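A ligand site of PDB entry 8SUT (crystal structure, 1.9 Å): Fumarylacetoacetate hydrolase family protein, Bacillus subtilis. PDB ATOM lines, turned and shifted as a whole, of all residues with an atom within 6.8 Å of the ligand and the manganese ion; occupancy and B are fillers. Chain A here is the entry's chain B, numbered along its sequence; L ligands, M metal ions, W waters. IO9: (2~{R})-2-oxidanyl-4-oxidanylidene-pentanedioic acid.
The manganese ion is bound by O04 of the ligand, O06 of the ligand, OD2 of Asp 182, water W1, OE1 of Glu 151 and OE2 of Glu 153.
O of Ile 100 sits close to O04 of the ligand (3.5 Å). Gly 101 touches the ligand (CA to C04, 3.6 Å). CD2 of His 107 touches O03 of the ligand (3.4 Å). Met 111 touches the ligand. Phe 124 touches the ligand. Phe 195 touches the ligand (CE2 to C01, 3.996 Å). Gly 268 touches the ligand. Hydrophobic or aromatic side chains that line the ligand: His 107, Met 111, Phe 124 and Phe 195. Of the 25 residues printed, 15 come within 4 Å of the ligand. The nearest printed residue that does not touch the ligand is Thr 184 (4.5 Å).
An oxygen (O05) of the ligand is in hydrogen-bond range of the side-chain amino group (NZ) of Lys 199, at 2.9 Å. N of Lys 102 lies within hydrogen-bond range of O03 of the ligand, 3.2 Å away. The side-chain amino group of Lys 102 lies within salt-bridge range of an oxygen (O02) of the ligand. O01 of the ligand lies within salt-bridge range of NH1 of Arg 186, 3.5 Å away. NE2 of Gln 189 sits at hydrogen-bond distance from O01 of the ligand, at 3.1 Å. N of Thr 269 lies close to O04 of the ligand, 3.2 Å away.
Water W1 lies within hydrogen-bond range of OE1 of Glu 153 (2.7 Å) and O of Ile 100 (2.7 Å).
O of Asp 182 is in hydrogen-bond range of OG1 of Thr 184, at 2.8 Å. The side-chain carboxylate (OE2) of Glu 151 is in salt-bridge range of the guanidinium group (NH2) of Arg 186 (2.7 Å). The side-chain carboxylate (OE1) of Glu 153 is in hydrogen-bond range of the backbone NH (N) of Gly 268, 2.9 Å away. OG1 of Thr 184 lies within hydrogen-bond range of NZ of Lys 199. The guanidinium group (NH1) of Arg 186 sits at hydrogen-bond distance from the side-chain amide oxygen (OE1) of Gln 189 (3.1 Å). The side-chain hydroxyl (OG1) of Thr 269 sits at hydrogen-bond distance from the backbone carbonyl oxygen (O) of Gly 152, at 2.8 Å. The backbone NH of Cys 99 sits at hydrogen-bond distance from the backbone carbonyl oxygen of Phe 124 (2.7 Å). The backbone carbonyl oxygen (O) of Met 122 lies within hydrogen-bond range of the backbone NH (N) of Gly 101, 2.8 Å away.
Residues that only touch the manganese ion: Lys 199 and Ile 100. Of the 25 residues printed, 5 come within 4 Å of the manganese ion. The nearest printed residue that does not touch the manganese ion is Phe 124 (4.2 Å).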
ATOM      1  N   CYS A  99      13.733 -11.385  11.575  1.00  0.00           N
ATOM      2  CA  CYS A  99      13.012 -12.493  10.956  1.00  0.00           C
ATOM      3  C   CYS A  99      13.068 -12.386   9.436  1.00  0.00           C
ATOM      4  O   CYS A  99      12.875 -11.314   8.862  1.00  0.00           O
ATOM      5  CB  CYS A  99      11.570 -12.553  11.417  1.00  0.00           C
ATOM      6  SG  CYS A  99      11.374 -12.839  13.194  1.00  0.00           S
ATOM      7  N   ILE A 100      13.324 -13.529   8.789  1.00  0.00           N
ATOM      8  CA  ILE A 100      13.264 -13.654   7.345  1.00  0.00           C
ATOM      9  C   ILE A 100      11.917 -14.252   6.974  1.00  0.00           C
ATOM     10  O   ILE A 100      11.475 -15.244   7.552  1.00  0.00           O
ATOM     11  CB  ILE A 100      14.446 -14.497   6.828  1.00  0.00           C
ATOM     12  CG1 ILE A 100      15.783 -14.118   7.522  1.00  0.00           C
ATOM     13  CG2 ILE A 100      14.563 -14.386   5.304  1.00  0.00           C
ATOM     14  CD1 ILE A 100      16.220 -12.626   7.386  1.00  0.00           C
ATOM     15  N   GLY A 101      11.246 -13.604   6.014  1.00  0.00           N
ATOM     16  CA  GLY A 101      10.045 -14.155   5.398  1.00  0.00           C
ATOM     17  C   GLY A 101      10.345 -14.888   4.096  1.00  0.00           C
ATOM     18  O   GLY A 101      11.258 -14.518   3.364  1.00  0.00           O
ATOM     19  N   LYS A 102       9.551 -15.925   3.801  1.00  0.00           N
ATOM     20  CA  LYS A 102       9.593 -16.612   2.513  1.00  0.00           C
ATOM     21  C   LYS A 102      11.009 -17.008   2.112  1.00  0.00           C
ATOM     22  O   LYS A 102      11.537 -16.534   1.111  1.00  0.00           O
ATOM     23  CB  LYS A 102       8.986 -15.693   1.425  1.00  0.00           C
ATOM     24  CG  LYS A 102       7.546 -15.247   1.691  1.00  0.00           C
ATOM     25  CD  LYS A 102       7.058 -14.251   0.631  1.00  0.00           C
ATOM     26  CE  LYS A 102       5.556 -14.219   0.542  1.00  0.00           C
ATOM     27  NZ  LYS A 102       4.933 -13.847   1.841  1.00  0.00           N
ATOM     28  N   ASN A 103      11.636 -17.864   2.926  1.00  0.00           N
ATOM     29  CA  ASN A 103      12.990 -18.324   2.640  1.00  0.00           C
ATOM     30  C   ASN A 103      13.005 -19.812   2.274  1.00  0.00           C
ATOM     31  O   ASN A 103      14.078 -20.384   2.080  1.00  0.00           O
ATOM     32  CB  ASN A 103      13.918 -18.023   3.836  1.00  0.00           C
ATOM     33  CG  ASN A 103      15.376 -18.023   3.471  1.00  0.00           C
ATOM     34  OD1 ASN A 103      15.730 -17.688   2.355  1.00  0.00           O
ATOM     35  ND2 ASN A 103      16.268 -18.437   4.396  1.00  0.00           N
ATOM     36  N   TYR A 104      11.818 -20.420   2.177  1.00  0.00           N
ATOM     37  CA  TYR A 104      11.647 -21.753   1.610  1.00  0.00           C
ATOM     38  C   TYR A 104      10.594 -21.658   0.497  1.00  0.00           C
ATOM     39  O   TYR A 104       9.512 -21.093   0.727  1.00  0.00           O
ATOM     40  CB  TYR A 104      11.163 -22.781   2.672  1.00  0.00           C
ATOM     41  CG  TYR A 104      12.154 -23.171   3.748  1.00  0.00           C
ATOM     42  CD1 TYR A 104      12.471 -22.293   4.781  1.00  0.00           C
ATOM     43  CD2 TYR A 104      12.752 -24.422   3.751  1.00  0.00           C
ATOM     44  CE1 TYR A 104      13.373 -22.647   5.783  1.00  0.00           C
ATOM     45  CE2 TYR A 104      13.658 -24.794   4.757  1.00  0.00           C
ATOM     46  CZ  TYR A 104      13.957 -23.905   5.770  1.00  0.00           C
ATOM     47  OH  TYR A 104      14.835 -24.230   6.781  1.00  0.00           O
ATOM     48  N   HIS A 107       6.865 -22.729   1.189  1.00  0.00           N
ATOM     49  CA  HIS A 107       6.173 -21.842   2.115  1.00  0.00           C
ATOM     50  C   HIS A 107       5.604 -20.634   1.366  1.00  0.00           C
ATOM     51  O   HIS A 107       4.446 -20.258   1.577  1.00  0.00           O
ATOM     52  CB  HIS A 107       7.071 -21.339   3.254  1.00  0.00           C
ATOM     53  CG  HIS A 107       6.319 -20.428   4.166  1.00  0.00           C
ATOM     54  ND1 HIS A 107       5.204 -20.879   4.837  1.00  0.00           N
ATOM     55  CD2 HIS A 107       6.440 -19.126   4.487  1.00  0.00           C
ATOM     56  CE1 HIS A 107       4.689 -19.890   5.549  1.00  0.00           C
ATOM     57  NE2 HIS A 107       5.419 -18.811   5.360  1.00  0.00           N
ATOM     58  N   ALA A 108       6.443 -20.009   0.532  1.00  0.00           N
ATOM     59  CA  ALA A 108       6.055 -18.879  -0.300  1.00  0.00           C
ATOM     60  C   ALA A 108       4.881 -19.214  -1.221  1.00  0.00           C
ATOM     61  O   ALA A 108       3.971 -18.396  -1.391  1.00  0.00           O
ATOM     62  CB  ALA A 108       7.257 -18.414  -1.109  1.00  0.00           C
ATOM     63  N   MET A 111       1.442 -19.683   0.570  1.00  0.00           N
ATOM     64  CA  MET A 111       0.929 -18.416   1.051  1.00  0.00           C
ATOM     65  C   MET A 111       0.420 -17.524  -0.082  1.00  0.00           C
ATOM     66  O   MET A 111      -0.080 -16.426   0.176  1.00  0.00           O
ATOM     67  CB  MET A 111       2.019 -17.663   1.861  1.00  0.00           C
ATOM     68  CG  MET A 111       2.436 -18.372   3.169  1.00  0.00           C
ATOM     69  SD  MET A 111       1.156 -18.428   4.470  1.00  0.00           S
ATOM     70  CE  MET A 111       0.810 -16.624   4.722  1.00  0.00           C
ATOM     71  N   MET A 122      13.131 -10.757   2.405  1.00  0.00           N
ATOM     72  CA  MET A 122      12.142  -9.941   3.077  1.00  0.00           C
ATOM     73  C   MET A 122      12.441 -10.062   4.574  1.00  0.00           C
ATOM     74  O   MET A 122      12.379 -11.158   5.127  1.00  0.00           O
ATOM     75  CB  MET A 122      10.748 -10.390   2.667  1.00  0.00           C
ATOM     76  CG  MET A 122       9.665 -10.101   3.687  1.00  0.00           C
ATOM     77  SD  MET A 122       8.056 -10.738   3.173  1.00  0.00           S
ATOM     78  CE  MET A 122       7.848  -9.884   1.613  1.00  0.00           C
ATOM     79  N   PHE A 124      11.824  -8.581   8.531  1.00  0.00           N
ATOM     80  CA  PHE A 124      11.037  -7.843   9.506  1.00  0.00           C
ATOM     81  C   PHE A 124      11.498  -8.262  10.898  1.00  0.00           C
ATOM     82  O   PHE A 124      12.461  -9.010  11.038  1.00  0.00           O
ATOM     83  CB  PHE A 124       9.546  -8.103   9.259  1.00  0.00           C
ATOM     84  CG  PHE A 124       9.217  -9.571   9.386  1.00  0.00           C
ATOM     85  CD1 PHE A 124       9.378 -10.428   8.306  1.00  0.00           C
ATOM     86  CD2 PHE A 124       8.832 -10.102  10.603  1.00  0.00           C
ATOM     87  CE1 PHE A 124       9.125 -11.782   8.439  1.00  0.00           C
ATOM     88  CE2 PHE A 124       8.567 -11.449  10.737  1.00  0.00           C
ATOM     89  CZ  PHE A 124       8.721 -12.277   9.651  1.00  0.00           C
ATOM     90  N   GLU A 151       5.042 -21.326  13.284  1.00  0.00           N
ATOM     91  CA  GLU A 151       6.128 -21.359  12.333  1.00  0.00           C
ATOM     92  C   GLU A 151       7.407 -21.848  13.002  1.00  0.00           C
ATOM     93  O   GLU A 151       8.060 -21.093  13.718  1.00  0.00           O
ATOM     94  CB  GLU A 151       6.385 -19.940  11.749  1.00  0.00           C
ATOM     95  CG  GLU A 151       5.191 -19.305  11.024  1.00  0.00           C
ATOM     96  CD  GLU A 151       5.584 -18.062  10.243  1.00  0.00           C
ATOM     97  OE1 GLU A 151       6.773 -17.684  10.347  1.00  0.00           O
ATOM     98  OE2 GLU A 151       4.754 -17.480   9.504  1.00  0.00           O
ATOM     99  N   GLY A 152       7.793 -23.091  12.733  1.00  0.00           N
ATOM    100  CA  GLY A 152       9.035 -23.627  13.274  1.00  0.00           C
ATOM    101  C   GLY A 152      10.197 -23.092  12.445  1.00  0.00           C
ATOM    102  O   GLY A 152      10.116 -23.111  11.231  1.00  0.00           O
ATOM    103  N   GLU A 153      11.252 -22.586  13.115  1.00  0.00           N
ATOM    104  CA  GLU A 153      12.403 -22.037  12.412  1.00  0.00           C
ATOM    105  C   GLU A 153      13.719 -22.257  13.129  1.00  0.00           C
ATOM    106  O   GLU A 153      13.771 -22.346  14.356  1.00  0.00           O
ATOM    107  CB  GLU A 153      12.270 -20.542  12.189  1.00  0.00           C
ATOM    108  CG  GLU A 153      10.897 -20.079  11.855  1.00  0.00           C
ATOM    109  CD  GLU A 153      10.791 -18.661  11.330  1.00  0.00           C
ATOM    110  OE1 GLU A 153      11.821 -17.972  11.092  1.00  0.00           O
ATOM    111  OE2 GLU A 153       9.639 -18.224  11.175  1.00  0.00           O
ATOM    112  N   ASP A 182       7.917 -18.793  15.413  1.00  0.00           N
ATOM    113  CA  ASP A 182       7.531 -17.448  15.010  1.00  0.00           C
ATOM    114  C   ASP A 182       6.011 -17.351  14.899  1.00  0.00           C
ATOM    115  O   ASP A 182       5.458 -17.260  13.803  1.00  0.00           O
ATOM    116  CB  ASP A 182       8.246 -17.065  13.707  1.00  0.00           C
ATOM    117  CG  ASP A 182       7.890 -15.700  13.113  1.00  0.00           C
ATOM    118  OD1 ASP A 182       7.277 -14.858  13.833  1.00  0.00           O
ATOM    119  OD2 ASP A 182       8.177 -15.500  11.930  1.00  0.00           O
ATOM    120  N   THR A 184       2.396 -16.081  14.712  1.00  0.00           N
ATOM    121  CA  THR A 184       1.953 -14.947  13.913  1.00  0.00           C
ATOM    122  C   THR A 184       0.427 -14.857  13.931  1.00  0.00           C
ATOM    123  O   THR A 184      -0.259 -15.872  13.819  1.00  0.00           O
ATOM    124  CB  THR A 184       2.442 -15.140  12.471  1.00  0.00           C
ATOM    125  OG1 THR A 184       3.863 -15.366  12.480  1.00  0.00           O
ATOM    126  CG2 THR A 184       2.089 -13.953  11.574  1.00  0.00           C
ATOM    127  N   ARG A 186      -2.226 -13.846  11.592  1.00  0.00           N
ATOM    128  CA  ARG A 186      -2.290 -13.669  10.144  1.00  0.00           C
ATOM    129  C   ARG A 186      -3.198 -12.532   9.690  1.00  0.00           C
ATOM    130  O   ARG A 186      -2.913 -11.873   8.694  1.00  0.00           O
ATOM    131  CB  ARG A 186      -2.781 -14.948   9.444  1.00  0.00           C
ATOM    132  CG  ARG A 186      -1.879 -16.152   9.632  1.00  0.00           C
ATOM    133  CD  ARG A 186      -0.627 -16.085   8.820  1.00  0.00           C
ATOM    134  NE  ARG A 186       0.241 -17.216   9.091  1.00  0.00           N
ATOM    135  CZ  ARG A 186       1.556 -17.216   8.896  1.00  0.00           C
ATOM    136  NH1 ARG A 186       2.197 -16.127   8.502  1.00  0.00           N
ATOM    137  NH2 ARG A 186       2.249 -18.338   9.108  1.00  0.00           N
ATOM    138  N   GLN A 189      -1.317  -9.286  10.331  1.00  0.00           N
ATOM    139  CA  GLN A 189      -0.384  -9.103   9.232  1.00  0.00           C
ATOM    140  C   GLN A 189      -1.003  -8.410   8.026  1.00  0.00           C
ATOM    141  O   GLN A 189      -0.390  -7.496   7.483  1.00  0.00           O
ATOM    142  CB  GLN A 189       0.165 -10.430   8.727  1.00  0.00           C
ATOM    143  CG  GLN A 189       1.362 -10.970   9.448  1.00  0.00           C
ATOM    144  CD  GLN A 189       1.865 -12.180   8.700  1.00  0.00           C
ATOM    145  OE1 GLN A 189       1.159 -13.185   8.558  1.00  0.00           O
ATOM    146  NE2 GLN A 189       3.081 -12.101   8.189  1.00  0.00           N
ATOM    147  N   PHE A 195       4.576  -6.289   8.903  1.00  0.00           N
ATOM    148  CA  PHE A 195       4.351  -7.461   9.733  1.00  0.00           C
ATOM    149  C   PHE A 195       4.532  -7.273  11.240  1.00  0.00           C
ATOM    150  O   PHE A 195       4.099  -8.126  12.023  1.00  0.00           O
ATOM    151  CB  PHE A 195       5.302  -8.579   9.265  1.00  0.00           C
ATOM    152  CG  PHE A 195       4.990  -9.195   7.919  1.00  0.00           C
ATOM    153  CD1 PHE A 195       3.849  -8.840   7.202  1.00  0.00           C
ATOM    154  CD2 PHE A 195       5.836 -10.146   7.367  1.00  0.00           C
ATOM    155  CE1 PHE A 195       3.575  -9.406   5.952  1.00  0.00           C
ATOM    156  CE2 PHE A 195       5.549 -10.732   6.135  1.00  0.00           C
ATOM    157  CZ  PHE A 195       4.429 -10.347   5.437  1.00  0.00           C
ATOM    158  N   LYS A 199       3.365  -9.914  14.257  1.00  0.00           N
ATOM    159  CA  LYS A 199       4.501 -10.694  14.705  1.00  0.00           C
ATOM    160  C   LYS A 199       4.915 -10.431  16.151  1.00  0.00           C
ATOM    161  O   LYS A 199       5.687 -11.203  16.699  1.00  0.00           O
ATOM    162  CB  LYS A 199       5.695 -10.398  13.794  1.00  0.00           C
ATOM    163  CG  LYS A 199       5.529 -10.890  12.373  1.00  0.00           C
ATOM    164  CD  LYS A 199       5.660 -12.379  12.277  1.00  0.00           C
ATOM    165  CE  LYS A 199       5.532 -12.863  10.846  1.00  0.00           C
ATOM    166  NZ  LYS A 199       5.831 -14.315  10.735  1.00  0.00           N
ATOM    167  N   ALA A 266      15.972 -15.309  12.936  1.00  0.00           N
ATOM    168  CA  ALA A 266      15.088 -16.401  12.581  1.00  0.00           C
ATOM    169  C   ALA A 266      15.019 -16.535  11.057  1.00  0.00           C
ATOM    170  O   ALA A 266      14.602 -15.588  10.385  1.00  0.00           O
ATOM    171  CB  ALA A 266      13.719 -16.155  13.168  1.00  0.00           C
ATOM    172  N   THR A 267      15.436 -17.699  10.527  1.00  0.00           N
ATOM    173  CA  THR A 267      15.769 -17.849   9.119  1.00  0.00           C
ATOM    174  C   THR A 267      14.627 -18.301   8.200  1.00  0.00           C
ATOM    175  O   THR A 267      14.841 -18.569   7.018  1.00  0.00           O
ATOM    176  CB  THR A 267      16.967 -18.801   9.017  1.00  0.00           C
ATOM    177  OG1 THR A 267      16.611 -20.093   9.517  1.00  0.00           O
ATOM    178  CG2 THR A 267      18.175 -18.261   9.772  1.00  0.00           C
ATOM    179  N   GLY A 268      13.404 -18.367   8.731  1.00  0.00           N
ATOM    180  CA  GLY A 268      12.238 -18.646   7.920  1.00  0.00           C
ATOM    181  C   GLY A 268      11.718 -20.064   8.151  1.00  0.00           C
ATOM    182  O   GLY A 268      12.484 -20.969   8.470  1.00  0.00           O
ATOM    183  N   THR A 269      10.405 -20.215   7.973  1.00  0.00           N
ATOM    184  CA  THR A 269       9.705 -21.471   8.233  1.00  0.00           C
ATOM    185  C   THR A 269       9.460 -22.220   6.928  1.00  0.00           C
ATOM    186  O   THR A 269       9.225 -21.600   5.889  1.00  0.00           O
ATOM    187  CB  THR A 269       8.422 -21.158   8.995  1.00  0.00           C
ATOM    188  OG1 THR A 269       7.946 -22.336   9.629  1.00  0.00           O
ATOM    189  CG2 THR A 269       7.299 -20.584   8.100  1.00  0.00           C
ATOM    190  N   PRO A 270       9.520 -23.579   6.931  1.00  0.00           N
ATOM    191  CA  PRO A 270       9.094 -24.354   5.758  1.00  0.00           C
ATOM    192  C   PRO A 270       7.582 -24.289   5.536  1.00  0.00           C
ATOM    193  O   PRO A 270       6.844 -23.653   6.316  1.00  0.00           O
ATOM    194  CB  PRO A 270       9.511 -25.788   6.102  1.00  0.00           C
ATOM    195  CG  PRO A 270      10.233 -25.719   7.425  1.00  0.00           C
ATOM    196  CD  PRO A 270       9.954 -24.417   8.056  1.00  0.00           C
HETATM  197  C01 IO9 L   1       4.626 -14.596   5.707  1.00  0.00           C
HETATM  198  C02 IO9 L   1       8.443 -16.883   7.635  1.00  0.00           C
HETATM  199  C03 IO9 L   1       5.400 -15.231   6.864  1.00  0.00           C
HETATM  200  C04 IO9 L   1       6.877 -14.858   6.862  1.00  0.00           C
HETATM  201  C05 IO9 L   1       7.624 -15.618   7.952  1.00  0.00           C
HETATM  202  O01 IO9 L   1       3.429 -14.198   5.868  1.00  0.00           O
HETATM  203  O02 IO9 L   1       5.187 -14.474   4.590  1.00  0.00           O
HETATM  204  O03 IO9 L   1       8.556 -17.331   6.458  1.00  0.00           O
HETATM  205  O04 IO9 L   1       9.009 -17.422   8.633  1.00  0.00           O
HETATM  206  O05 IO9 L   1       4.847 -14.785   8.085  1.00  0.00           O
HETATM  207  O06 IO9 L   1       7.615 -15.307   9.109  1.00  0.00           O
HETATM  208 MN    MN M   1       8.655 -16.423  10.068  1.00  0.00          MN
HETATM  209  O   HOH W   1      10.678 -15.740  10.119  1.00  0.00           O
